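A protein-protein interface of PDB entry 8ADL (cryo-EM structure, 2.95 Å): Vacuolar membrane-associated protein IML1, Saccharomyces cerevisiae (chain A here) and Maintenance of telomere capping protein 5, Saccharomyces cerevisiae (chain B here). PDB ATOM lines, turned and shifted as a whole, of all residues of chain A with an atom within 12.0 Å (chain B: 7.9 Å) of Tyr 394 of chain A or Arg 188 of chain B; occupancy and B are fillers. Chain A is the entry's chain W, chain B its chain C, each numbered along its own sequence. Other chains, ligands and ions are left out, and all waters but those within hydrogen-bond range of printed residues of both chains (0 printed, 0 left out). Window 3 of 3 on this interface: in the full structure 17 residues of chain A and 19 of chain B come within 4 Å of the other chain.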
ATOM      1  N   LYS A 383      -4.599 -24.228  10.596  1.00  0.00           N
ATOM      2  CA  LYS A 383      -3.684 -23.164  10.995  1.00  0.00           C
ATOM      3  C   LYS A 383      -2.263 -23.442  10.520  1.00  0.00           C
ATOM      4  O   LYS A 383      -1.531 -22.506  10.173  1.00  0.00           O
ATOM      5  CB  LYS A 383      -3.718 -22.996  12.514  1.00  0.00           C
ATOM      6  CG  LYS A 383      -2.937 -21.806  13.046  1.00  0.00           C
ATOM      7  CD  LYS A 383      -2.896 -21.812  14.566  1.00  0.00           C
ATOM      8  CE  LYS A 383      -2.739 -20.404  15.119  1.00  0.00           C
ATOM      9  NZ  LYS A 383      -1.949 -19.529  14.210  1.00  0.00           N
ATOM     10  N   LEU A 385      -1.289 -25.029   7.752  1.00  0.00           N
ATOM     11  CA  LEU A 385      -1.099 -24.940   6.308  1.00  0.00           C
ATOM     12  C   LEU A 385      -1.632 -23.655   5.690  1.00  0.00           C
ATOM     13  O   LEU A 385      -0.950 -23.052   4.856  1.00  0.00           O
ATOM     14  CB  LEU A 385      -1.762 -26.132   5.618  1.00  0.00           C
ATOM     15  CG  LEU A 385      -1.099 -27.477   5.880  1.00  0.00           C
ATOM     16  CD1 LEU A 385      -2.047 -28.580   5.505  1.00  0.00           C
ATOM     17  CD2 LEU A 385       0.174 -27.572   5.067  1.00  0.00           C
ATOM     18  N   LEU A 386      -2.826 -23.217   6.070  1.00  0.00           N
ATOM     19  CA  LEU A 386      -3.472 -22.096   5.406  1.00  0.00           C
ATOM     20  C   LEU A 386      -3.033 -20.744   5.955  1.00  0.00           C
ATOM     21  O   LEU A 386      -3.553 -19.715   5.513  1.00  0.00           O
ATOM     22  CB  LEU A 386      -4.992 -22.247   5.511  1.00  0.00           C
ATOM     23  CG  LEU A 386      -5.541 -23.508   4.834  1.00  0.00           C
ATOM     24  CD1 LEU A 386      -7.055 -23.559   4.903  1.00  0.00           C
ATOM     25  CD2 LEU A 386      -5.078 -23.590   3.392  1.00  0.00           C
ATOM     26  N   ASN A 387      -2.104 -20.722   6.906  1.00  0.00           N
ATOM     27  CA  ASN A 387      -1.530 -19.491   7.443  1.00  0.00           C
ATOM     28  C   ASN A 387      -0.057 -19.445   7.046  1.00  0.00           C
ATOM     29  O   ASN A 387       0.818 -19.864   7.806  1.00  0.00           O
ATOM     30  CB  ASN A 387      -1.700 -19.415   8.958  1.00  0.00           C
ATOM     31  CG  ASN A 387      -2.101 -18.031   9.430  1.00  0.00           C
ATOM     32  OD1 ASN A 387      -2.769 -17.286   8.711  1.00  0.00           O
ATOM     33  ND2 ASN A 387      -1.694 -17.680  10.643  1.00  0.00           N
ATOM     34  N   LYS A 388       0.214 -18.933   5.849  1.00  0.00           N
ATOM     35  CA  LYS A 388       1.584 -18.843   5.371  1.00  0.00           C
ATOM     36  C   LYS A 388       2.300 -17.677   6.041  1.00  0.00           C
ATOM     37  O   LYS A 388       1.676 -16.719   6.507  1.00  0.00           O
ATOM     38  CB  LYS A 388       1.633 -18.677   3.850  1.00  0.00           C
ATOM     39  CG  LYS A 388       1.276 -17.283   3.353  1.00  0.00           C
ATOM     40  CD  LYS A 388       1.396 -17.171   1.846  1.00  0.00           C
ATOM     41  CE  LYS A 388       1.269 -15.722   1.401  1.00  0.00           C
ATOM     42  NZ  LYS A 388       1.390 -15.577  -0.075  1.00  0.00           N
ATOM     43  N   GLN A 389       3.622 -17.780   6.112  1.00  0.00           N
ATOM     44  CA  GLN A 389       4.449 -16.780   6.773  1.00  0.00           C
ATOM     45  C   GLN A 389       5.096 -15.898   5.712  1.00  0.00           C
ATOM     46  O   GLN A 389       5.817 -16.396   4.840  1.00  0.00           O
ATOM     47  CB  GLN A 389       5.513 -17.442   7.648  1.00  0.00           C
ATOM     48  CG  GLN A 389       6.407 -16.465   8.391  1.00  0.00           C
ATOM     49  CD  GLN A 389       5.662 -15.689   9.459  1.00  0.00           C
ATOM     50  OE1 GLN A 389       4.777 -16.223  10.127  1.00  0.00           O
ATOM     51  NE2 GLN A 389       6.020 -14.421   9.627  1.00  0.00           N
ATOM     52  N   THR A 390       4.836 -14.597   5.787  1.00  0.00           N
ATOM     53  CA  THR A 390       5.444 -13.632   4.885  1.00  0.00           C
ATOM     54  C   THR A 390       6.697 -13.049   5.532  1.00  0.00           C
ATOM     55  O   THR A 390       6.774 -12.901   6.754  1.00  0.00           O
ATOM     56  CB  THR A 390       4.444 -12.522   4.541  1.00  0.00           C
ATOM     57  OG1 THR A 390       3.157 -13.103   4.306  1.00  0.00           O
ATOM     58  CG2 THR A 390       4.865 -11.766   3.284  1.00  0.00           C
ATOM     59  N   ASP A 391       7.686 -12.721   4.696  1.00  0.00           N
ATOM     60  CA  ASP A 391       8.964 -12.210   5.184  1.00  0.00           C
ATOM     61  C   ASP A 391       8.874 -10.796   5.746  1.00  0.00           C
ATOM     62  O   ASP A 391       9.851 -10.324   6.337  1.00  0.00           O
ATOM     63  CB  ASP A 391      10.003 -12.249   4.061  1.00  0.00           C
ATOM     64  CG  ASP A 391      10.157 -13.631   3.458  1.00  0.00           C
ATOM     65  OD1 ASP A 391       9.489 -14.570   3.941  1.00  0.00           O
ATOM     66  OD2 ASP A 391      10.946 -13.780   2.502  1.00  0.00           O
ATOM     67  N   LYS A 392       7.742 -10.111   5.580  1.00  0.00           N
ATOM     68  CA  LYS A 392       7.567  -8.754   6.084  1.00  0.00           C
ATOM     69  C   LYS A 392       7.286  -8.698   7.581  1.00  0.00           C
ATOM     70  O   LYS A 392       7.100  -7.599   8.116  1.00  0.00           O
ATOM     71  CB  LYS A 392       6.437  -8.052   5.327  1.00  0.00           C
ATOM     72  CG  LYS A 392       6.488  -8.222   3.818  1.00  0.00           C
ATOM     73  CD  LYS A 392       5.340  -7.482   3.151  1.00  0.00           C
ATOM     74  CE  LYS A 392       5.525  -7.409   1.646  1.00  0.00           C
ATOM     75  NZ  LYS A 392       4.467  -6.584   1.001  1.00  0.00           N
ATOM     76  N   GLY A 393       7.249  -9.835   8.269  1.00  0.00           N
ATOM     77  CA  GLY A 393       7.029  -9.859   9.699  1.00  0.00           C
ATOM     78  C   GLY A 393       5.640 -10.255  10.149  1.00  0.00           C
ATOM     79  O   GLY A 393       5.363 -10.198  11.353  1.00  0.00           O
ATOM     80  N   TYR A 394       4.762 -10.653   9.231  1.00  0.00           N
ATOM     81  CA  TYR A 394       3.407 -11.052   9.582  1.00  0.00           C
ATOM     82  C   TYR A 394       2.985 -12.231   8.715  1.00  0.00           C
ATOM     83  O   TYR A 394       3.664 -12.602   7.756  1.00  0.00           O
ATOM     84  CB  TYR A 394       2.423  -9.880   9.446  1.00  0.00           C
ATOM     85  CG  TYR A 394       2.341  -9.255   8.066  1.00  0.00           C
ATOM     86  CD1 TYR A 394       1.439  -9.724   7.116  1.00  0.00           C
ATOM     87  CD2 TYR A 394       3.149  -8.178   7.726  1.00  0.00           C
ATOM     88  CE1 TYR A 394       1.359  -9.149   5.862  1.00  0.00           C
ATOM     89  CE2 TYR A 394       3.072  -7.595   6.474  1.00  0.00           C
ATOM     90  CZ  TYR A 394       2.177  -8.085   5.547  1.00  0.00           C
ATOM     91  OH  TYR A 394       2.100  -7.509   4.300  1.00  0.00           O
ATOM     92  N   SER A 395       1.848 -12.822   9.068  1.00  0.00           N
ATOM     93  CA  SER A 395       1.344 -14.020   8.414  1.00  0.00           C
ATOM     94  C   SER A 395       0.070 -13.698   7.645  1.00  0.00           C
ATOM     95  O   SER A 395      -0.785 -12.948   8.124  1.00  0.00           O
ATOM     96  CB  SER A 395       1.069 -15.130   9.432  1.00  0.00           C
ATOM     97  OG  SER A 395       0.779 -16.356   8.782  1.00  0.00           O
ATOM     98  N   VAL A 396      -0.041 -14.261   6.444  1.00  0.00           N
ATOM     99  CA  VAL A 396      -1.162 -14.018   5.546  1.00  0.00           C
ATOM    100  C   VAL A 396      -1.940 -15.316   5.387  1.00  0.00           C
ATOM    101  O   VAL A 396      -1.354 -16.366   5.099  1.00  0.00           O
ATOM    102  CB  VAL A 396      -0.677 -13.491   4.182  1.00  0.00           C
ATOM    103  CG1 VAL A 396      -1.819 -13.439   3.178  1.00  0.00           C
ATOM    104  CG2 VAL A 396      -0.042 -12.121   4.342  1.00  0.00           C
ATOM    105  N   ALA A 397      -3.254 -15.246   5.585  1.00  0.00           N
ATOM    106  CA  ALA A 397      -4.125 -16.407   5.417  1.00  0.00           C
ATOM    107  C   ALA A 397      -4.251 -16.703   3.928  1.00  0.00           C
ATOM    108  O   ALA A 397      -5.075 -16.109   3.230  1.00  0.00           O
ATOM    109  CB  ALA A 397      -5.488 -16.153   6.051  1.00  0.00           C
ATOM    110  N   ASN A 398      -3.432 -17.630   3.435  1.00  0.00           N
ATOM    111  CA  ASN A 398      -3.384 -17.949   2.017  1.00  0.00           C
ATOM    112  C   ASN A 398      -3.221 -19.451   1.837  1.00  0.00           C
ATOM    113  O   ASN A 398      -2.790 -20.166   2.745  1.00  0.00           O
ATOM    114  CB  ASN A 398      -2.243 -17.204   1.311  1.00  0.00           C
ATOM    115  CG  ASN A 398      -2.496 -17.014  -0.172  1.00  0.00           C
ATOM    116  OD1 ASN A 398      -3.618 -17.184  -0.648  1.00  0.00           O
ATOM    117  ND2 ASN A 398      -1.449 -16.666  -0.911  1.00  0.00           N
ATOM    118  N   TYR B 152      -8.860  -8.890   1.922  1.00  0.00           N
ATOM    119  CA  TYR B 152      -8.212  -9.196   3.189  1.00  0.00           C
ATOM    120  C   TYR B 152      -8.871 -10.439   3.767  1.00  0.00           C
ATOM    121  O   TYR B 152     -10.102 -10.510   3.838  1.00  0.00           O
ATOM    122  CB  TYR B 152      -8.326  -8.018   4.162  1.00  0.00           C
ATOM    123  CG  TYR B 152      -7.752  -8.277   5.534  1.00  0.00           C
ATOM    124  CD1 TYR B 152      -6.377  -8.316   5.735  1.00  0.00           C
ATOM    125  CD2 TYR B 152      -8.582  -8.485   6.630  1.00  0.00           C
ATOM    126  CE1 TYR B 152      -5.845  -8.547   6.987  1.00  0.00           C
ATOM    127  CE2 TYR B 152      -8.059  -8.721   7.889  1.00  0.00           C
ATOM    128  CZ  TYR B 152      -6.690  -8.751   8.060  1.00  0.00           C
ATOM    129  OH  TYR B 152      -6.163  -8.985   9.309  1.00  0.00           O
ATOM    130  N   ASP B 170      -9.708   4.801  13.960  1.00  0.00           N
ATOM    131  CA  ASP B 170      -8.602   4.289  13.165  1.00  0.00           C
ATOM    132  C   ASP B 170      -9.210   3.429  12.063  1.00  0.00           C
ATOM    133  O   ASP B 170      -9.753   2.355  12.361  1.00  0.00           O
ATOM    134  CB  ASP B 170      -7.656   3.469  14.037  1.00  0.00           C
ATOM    135  CG  ASP B 170      -6.345   3.120  13.342  1.00  0.00           C
ATOM    136  OD1 ASP B 170      -6.151   3.493  12.169  1.00  0.00           O
ATOM    137  OD2 ASP B 170      -5.497   2.464  13.983  1.00  0.00           O
ATOM    138  N   PRO B 171      -9.145   3.844  10.792  1.00  0.00           N
ATOM    139  CA  PRO B 171      -9.986   3.217   9.761  1.00  0.00           C
ATOM    140  C   PRO B 171      -9.449   1.916   9.176  1.00  0.00           C
ATOM    141  O   PRO B 171      -9.914   1.488   8.116  1.00  0.00           O
ATOM    142  CB  PRO B 171     -10.085   4.305   8.681  1.00  0.00           C
ATOM    143  CG  PRO B 171      -9.094   5.382   9.057  1.00  0.00           C
ATOM    144  CD  PRO B 171      -8.311   4.922  10.239  1.00  0.00           C
ATOM    145  N   ASN B 172      -8.483   1.274   9.836  1.00  0.00           N
ATOM    146  CA  ASN B 172      -8.043  -0.042   9.385  1.00  0.00           C
ATOM    147  C   ASN B 172      -7.793  -0.988  10.554  1.00  0.00           C
ATOM    148  O   ASN B 172      -6.896  -1.836  10.488  1.00  0.00           O
ATOM    149  CB  ASN B 172      -6.787   0.058   8.515  1.00  0.00           C
ATOM    150  CG  ASN B 172      -5.749   0.994   9.094  1.00  0.00           C
ATOM    151  OD1 ASN B 172      -5.880   1.458  10.224  1.00  0.00           O
ATOM    152  ND2 ASN B 172      -4.712   1.279   8.318  1.00  0.00           N
ATOM    153  N   VAL B 173      -8.570  -0.863  11.626  1.00  0.00           N
ATOM    154  CA  VAL B 173      -8.496  -1.775  12.762  1.00  0.00           C
ATOM    155  C   VAL B 173      -9.881  -2.367  12.978  1.00  0.00           C
ATOM    156  O   VAL B 173     -10.860  -1.628  13.140  1.00  0.00           O
ATOM    157  CB  VAL B 173      -7.992  -1.067  14.031  1.00  0.00           C
ATOM    158  CG1 VAL B 173      -8.283  -1.904  15.271  1.00  0.00           C
ATOM    159  CG2 VAL B 173      -6.503  -0.779  13.920  1.00  0.00           C
ATOM    160  N   LEU B 174      -9.965  -3.696  12.969  1.00  0.00           N
ATOM    161  CA  LEU B 174     -11.221  -4.397  13.184  1.00  0.00           C
ATOM    162  C   LEU B 174     -10.987  -5.554  14.145  1.00  0.00           C
ATOM    163  O   LEU B 174      -9.910  -6.154  14.166  1.00  0.00           O
ATOM    164  CB  LEU B 174     -11.835  -4.919  11.868  1.00  0.00           C
ATOM    165  CG  LEU B 174     -11.233  -6.125  11.127  1.00  0.00           C
ATOM    166  CD1 LEU B 174     -12.234  -6.663  10.118  1.00  0.00           C
ATOM    167  CD2 LEU B 174      -9.919  -5.800  10.424  1.00  0.00           C
ATOM    168  N   TRP B 185      -7.746  -7.367  14.677  1.00  0.00           N
ATOM    169  CA  TRP B 185      -6.961  -7.483  13.457  1.00  0.00           C
ATOM    170  C   TRP B 185      -6.573  -6.101  12.945  1.00  0.00           C
ATOM    171  O   TRP B 185      -7.376  -5.164  12.977  1.00  0.00           O
ATOM    172  CB  TRP B 185      -7.730  -8.228  12.364  1.00  0.00           C
ATOM    173  CG  TRP B 185      -8.557  -9.379  12.842  1.00  0.00           C
ATOM    174  CD1 TRP B 185      -9.904  -9.389  13.041  1.00  0.00           C
ATOM    175  CD2 TRP B 185      -8.093 -10.694  13.172  1.00  0.00           C
ATOM    176  NE1 TRP B 185     -10.309 -10.627  13.475  1.00  0.00           N
ATOM    177  CE2 TRP B 185      -9.217 -11.446  13.565  1.00  0.00           C
ATOM    178  CE3 TRP B 185      -6.836 -11.307  13.176  1.00  0.00           C
ATOM    179  CZ2 TRP B 185      -9.124 -12.780  13.954  1.00  0.00           C
ATOM    180  CZ3 TRP B 185      -6.746 -12.632  13.567  1.00  0.00           C
ATOM    181  CH2 TRP B 185      -7.883 -13.354  13.950  1.00  0.00           C
ATOM    182  N   ASP B 186      -5.334  -5.986  12.474  1.00  0.00           N
ATOM    183  CA  ASP B 186      -4.871  -4.833  11.713  1.00  0.00           C
ATOM    184  C   ASP B 186      -4.888  -5.171  10.228  1.00  0.00           C
ATOM    185  O   ASP B 186      -4.397  -6.230   9.823  1.00  0.00           O
ATOM    186  CB  ASP B 186      -3.464  -4.418  12.147  1.00  0.00           C
ATOM    187  CG  ASP B 186      -3.137  -2.986  11.774  1.00  0.00           C
ATOM    188  OD1 ASP B 186      -3.998  -2.311  11.169  1.00  0.00           O
ATOM    189  OD2 ASP B 186      -2.014  -2.533  12.084  1.00  0.00           O
ATOM    190  N   LEU B 187      -5.461  -4.273   9.422  1.00  0.00           N
ATOM    191  CA  LEU B 187      -5.666  -4.559   8.006  1.00  0.00           C
ATOM    192  C   LEU B 187      -4.365  -4.576   7.209  1.00  0.00           C
ATOM    193  O   LEU B 187      -4.331  -5.153   6.118  1.00  0.00           O
ATOM    194  CB  LEU B 187      -6.621  -3.524   7.403  1.00  0.00           C
ATOM    195  CG  LEU B 187      -7.381  -3.869   6.120  1.00  0.00           C
ATOM    196  CD1 LEU B 187      -8.476  -4.884   6.397  1.00  0.00           C
ATOM    197  CD2 LEU B 187      -7.957  -2.614   5.482  1.00  0.00           C
ATOM    198  N   ARG B 188      -3.296  -3.975   7.728  1.00  0.00           N
ATOM    199  CA  ARG B 188      -1.986  -4.036   7.093  1.00  0.00           C
ATOM    200  C   ARG B 188      -1.062  -5.081   7.703  1.00  0.00           C
ATOM    201  O   ARG B 188       0.085  -5.202   7.259  1.00  0.00           O
ATOM    202  CB  ARG B 188      -1.311  -2.661   7.147  1.00  0.00           C
ATOM    203  CG  ARG B 188      -2.233  -1.505   6.806  1.00  0.00           C
ATOM    204  CD  ARG B 188      -1.804  -0.225   7.502  1.00  0.00           C
ATOM    205  NE  ARG B 188      -1.876  -0.339   8.954  1.00  0.00           N
ATOM    206  CZ  ARG B 188      -1.579   0.640   9.797  1.00  0.00           C
ATOM    207  NH1 ARG B 188      -1.166   1.822   9.369  1.00  0.00           N
ATOM    208  NH2 ARG B 188      -1.698   0.428  11.105  1.00  0.00           N
ATOM    209  N   LYS B 189      -1.521  -5.838   8.699  1.00  0.00           N
ATOM    210  CA  LYS B 189      -0.677  -6.816   9.376  1.00  0.00           C
ATOM    211  C   LYS B 189      -1.103  -8.254   9.101  1.00  0.00           C
ATOM    212  O   LYS B 189      -0.743  -9.156   9.864  1.00  0.00           O
ATOM    213  CB  LYS B 189      -0.651  -6.544  10.880  1.00  0.00           C
ATOM    214  CG  LYS B 189       0.180  -5.330  11.263  1.00  0.00           C
ATOM    215  CD  LYS B 189       0.458  -5.283  12.755  1.00  0.00           C
ATOM    216  CE  LYS B 189       1.359  -4.109  13.103  1.00  0.00           C
ATOM    217  NZ  LYS B 189       1.676  -4.052  14.556  1.00  0.00           N
ATOM    218  N   GLY B 190      -1.853  -8.484   8.024  1.00  0.00           N
ATOM    219  CA  GLY B 190      -2.194  -9.841   7.621  1.00  0.00           C
ATOM    220  C   GLY B 190      -3.115 -10.529   8.613  1.00  0.00           C
ATOM    221  O   GLY B 190      -4.017  -9.918   9.196  1.00  0.00           O
ATOM    222  N   SER B 191      -2.867 -11.819   8.829  1.00  0.00           N
ATOM    223  CA  SER B 191      -3.671 -12.620   9.740  1.00  0.00           C
ATOM    224  C   SER B 191      -3.166 -12.594  11.175  1.00  0.00           C
ATOM    225  O   SER B 191      -3.838 -13.135  12.060  1.00  0.00           O
ATOM    226  CB  SER B 191      -3.735 -14.072   9.252  1.00  0.00           C
ATOM    227  OG  SER B 191      -2.535 -14.764   9.552  1.00  0.00           O
ATOM    228  N   THR B 192      -2.011 -11.992  11.430  1.00  0.00           N
ATOM    229  CA  THR B 192      -1.499 -11.906  12.791  1.00  0.00           C
ATOM    230  C   THR B 192      -2.266 -10.837  13.559  1.00  0.00           C
ATOM    231  O   THR B 192      -2.315  -9.685  13.112  1.00  0.00           O
ATOM    232  CB  THR B 192      -0.011 -11.581  12.792  1.00  0.00           C
ATOM    233  OG1 THR B 192       0.237 -10.469  11.922  1.00  0.00           O
ATOM    234  CG2 THR B 192       0.799 -12.782  12.325  1.00  0.00           C
ATOM    235  N   PRO B 193      -2.875 -11.166  14.696  1.00  0.00           N
ATOM    236  CA  PRO B 193      -3.672 -10.171  15.419  1.00  0.00           C
ATOM    237  C   PRO B 193      -2.793  -9.156  16.133  1.00  0.00           C
ATOM    238  O   PRO B 193      -1.672  -9.453  16.553  1.00  0.00           O
ATOM    239  CB  PRO B 193      -4.473 -11.011  16.426  1.00  0.00           C
ATOM    240  CG  PRO B 193      -4.182 -12.459  16.093  1.00  0.00           C
ATOM    241  CD  PRO B 193      -2.880 -12.474  15.369  1.00  0.00           C
ATOM    242  N   LEU B 194      -3.317  -7.932  16.247  1.00  0.00           N
ATOM    243  CA  LEU B 194      -2.656  -6.918  17.063  1.00  0.00           C
ATOM    244  C   LEU B 194      -2.660  -7.315  18.533  1.00  0.00           C
ATOM    245  O   LEU B 194      -1.653  -7.150  19.232  1.00  0.00           O
ATOM    246  CB  LEU B 194      -3.335  -5.562  16.874  1.00  0.00           C
ATOM    247  CG  LEU B 194      -2.715  -4.612  15.850  1.00  0.00           C
ATOM    248  CD1 LEU B 194      -3.541  -3.342  15.733  1.00  0.00           C
ATOM    249  CD2 LEU B 194      -1.287  -4.284  16.236  1.00  0.00           C
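Of the 15 printed residues of chain A, 4 touch a printed residue of chain B. Hydrophobic or aromatic side chains of chain A that line the printed part of chain B: Tyr 394. Printed residues of chain B that touch a printed residue of chain A: Arg 188, Lys 189, Gly 190, Ser 191 and Thr 192. Among the printed residues, 9 pairs touch across the chains. Among the printed residues, no Asp or Glu carboxylate lies within 4 Å of a Lys or Arg side-chain nitrogen of the other chain.
CE2 of Tyr 394 of chain A touches O of Arg 188 of chain B (3.9 Å). CB of Tyr 394 of chain A touches O of Lys 189 of chain B, 3.3 Å away. Tyr 394 of chain A touches Gly 190 of chain B (CD1 to N, 3.6 Å). Tyr 394 of chain A touches Thr 192 of chain B. Ser 395 of chain A touches Gly 190 of chain B (O to C, 3.4 Å). Ser 395 of chain A touches Thr 192 of chain B. Ser 191 of chain B touches Ala 397 of chain A (CB to N, 3.9 Å).
Of the printed residues of chain A, Arg 188 of chain B touches Tyr 394 (3.9 Å). No residue of chain A comes within 4 Å of Asn 172 of chain B. No residue of chain A comes within 4 Å of Asp 186 of chain B. Leu 187 of chain B touches none of the printed residues of chain A. Gly 190 of chain B touches just these residues of chain A: Tyr 394 (3.6 Å) and Ser 395 (3.4 Å). Of chain A, only Tyr 394 and Ser 395 come within 4 Å of Thr 192 of chain B. Of the printed residues of chain B, Asn 387 of chain A touches Ser 191. Printed residues of chain B within 4 Å of Ser 395 of chain A: Gly 190, Ser 191 and Thr 192. Leu 385 of chain A touches none of the printed residues of chain B. Trp 185 of chain B touches none of the printed residues of chain A. The nearest residue of chain A that does not touch Arg 188 of chain B is Lys 392 of chain A (7.0 Å).
The side-chain amide oxygen of Asn 387 of chain A is in hydrogen-bond range of the side-chain hydroxyl of Ser 191 of chain B. N of Ser 191 of chain B is in hydrogen-bond range of O of Ser 395 of chain A (2.5 Å).
The guanidinium group (NE) of Arg 188 of chain B lies close to the side-chain amide nitrogen (ND2) of Asn 172 of chain B (3.3 Å). ND2 of Asn 387 of chain A sits at hydrogen-bond distance from OG of Ser 395 of chain A (3.4 Å). OD2 of Asp 186 of chain B is in salt-bridge range of NH2 of Arg 188 of chain B. The backbone carbonyl oxygen of Lys 388 of chain A lies within hydrogen-bond range of the side-chain hydroxyl of Ser 395 of chain A, at 2.5 Å. The backbone carbonyl oxygen (O) of Lys 189 of chain B lies within hydrogen-bond range of the side-chain hydroxyl (OG1) of Thr 192 of chain B (2.6 Å).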
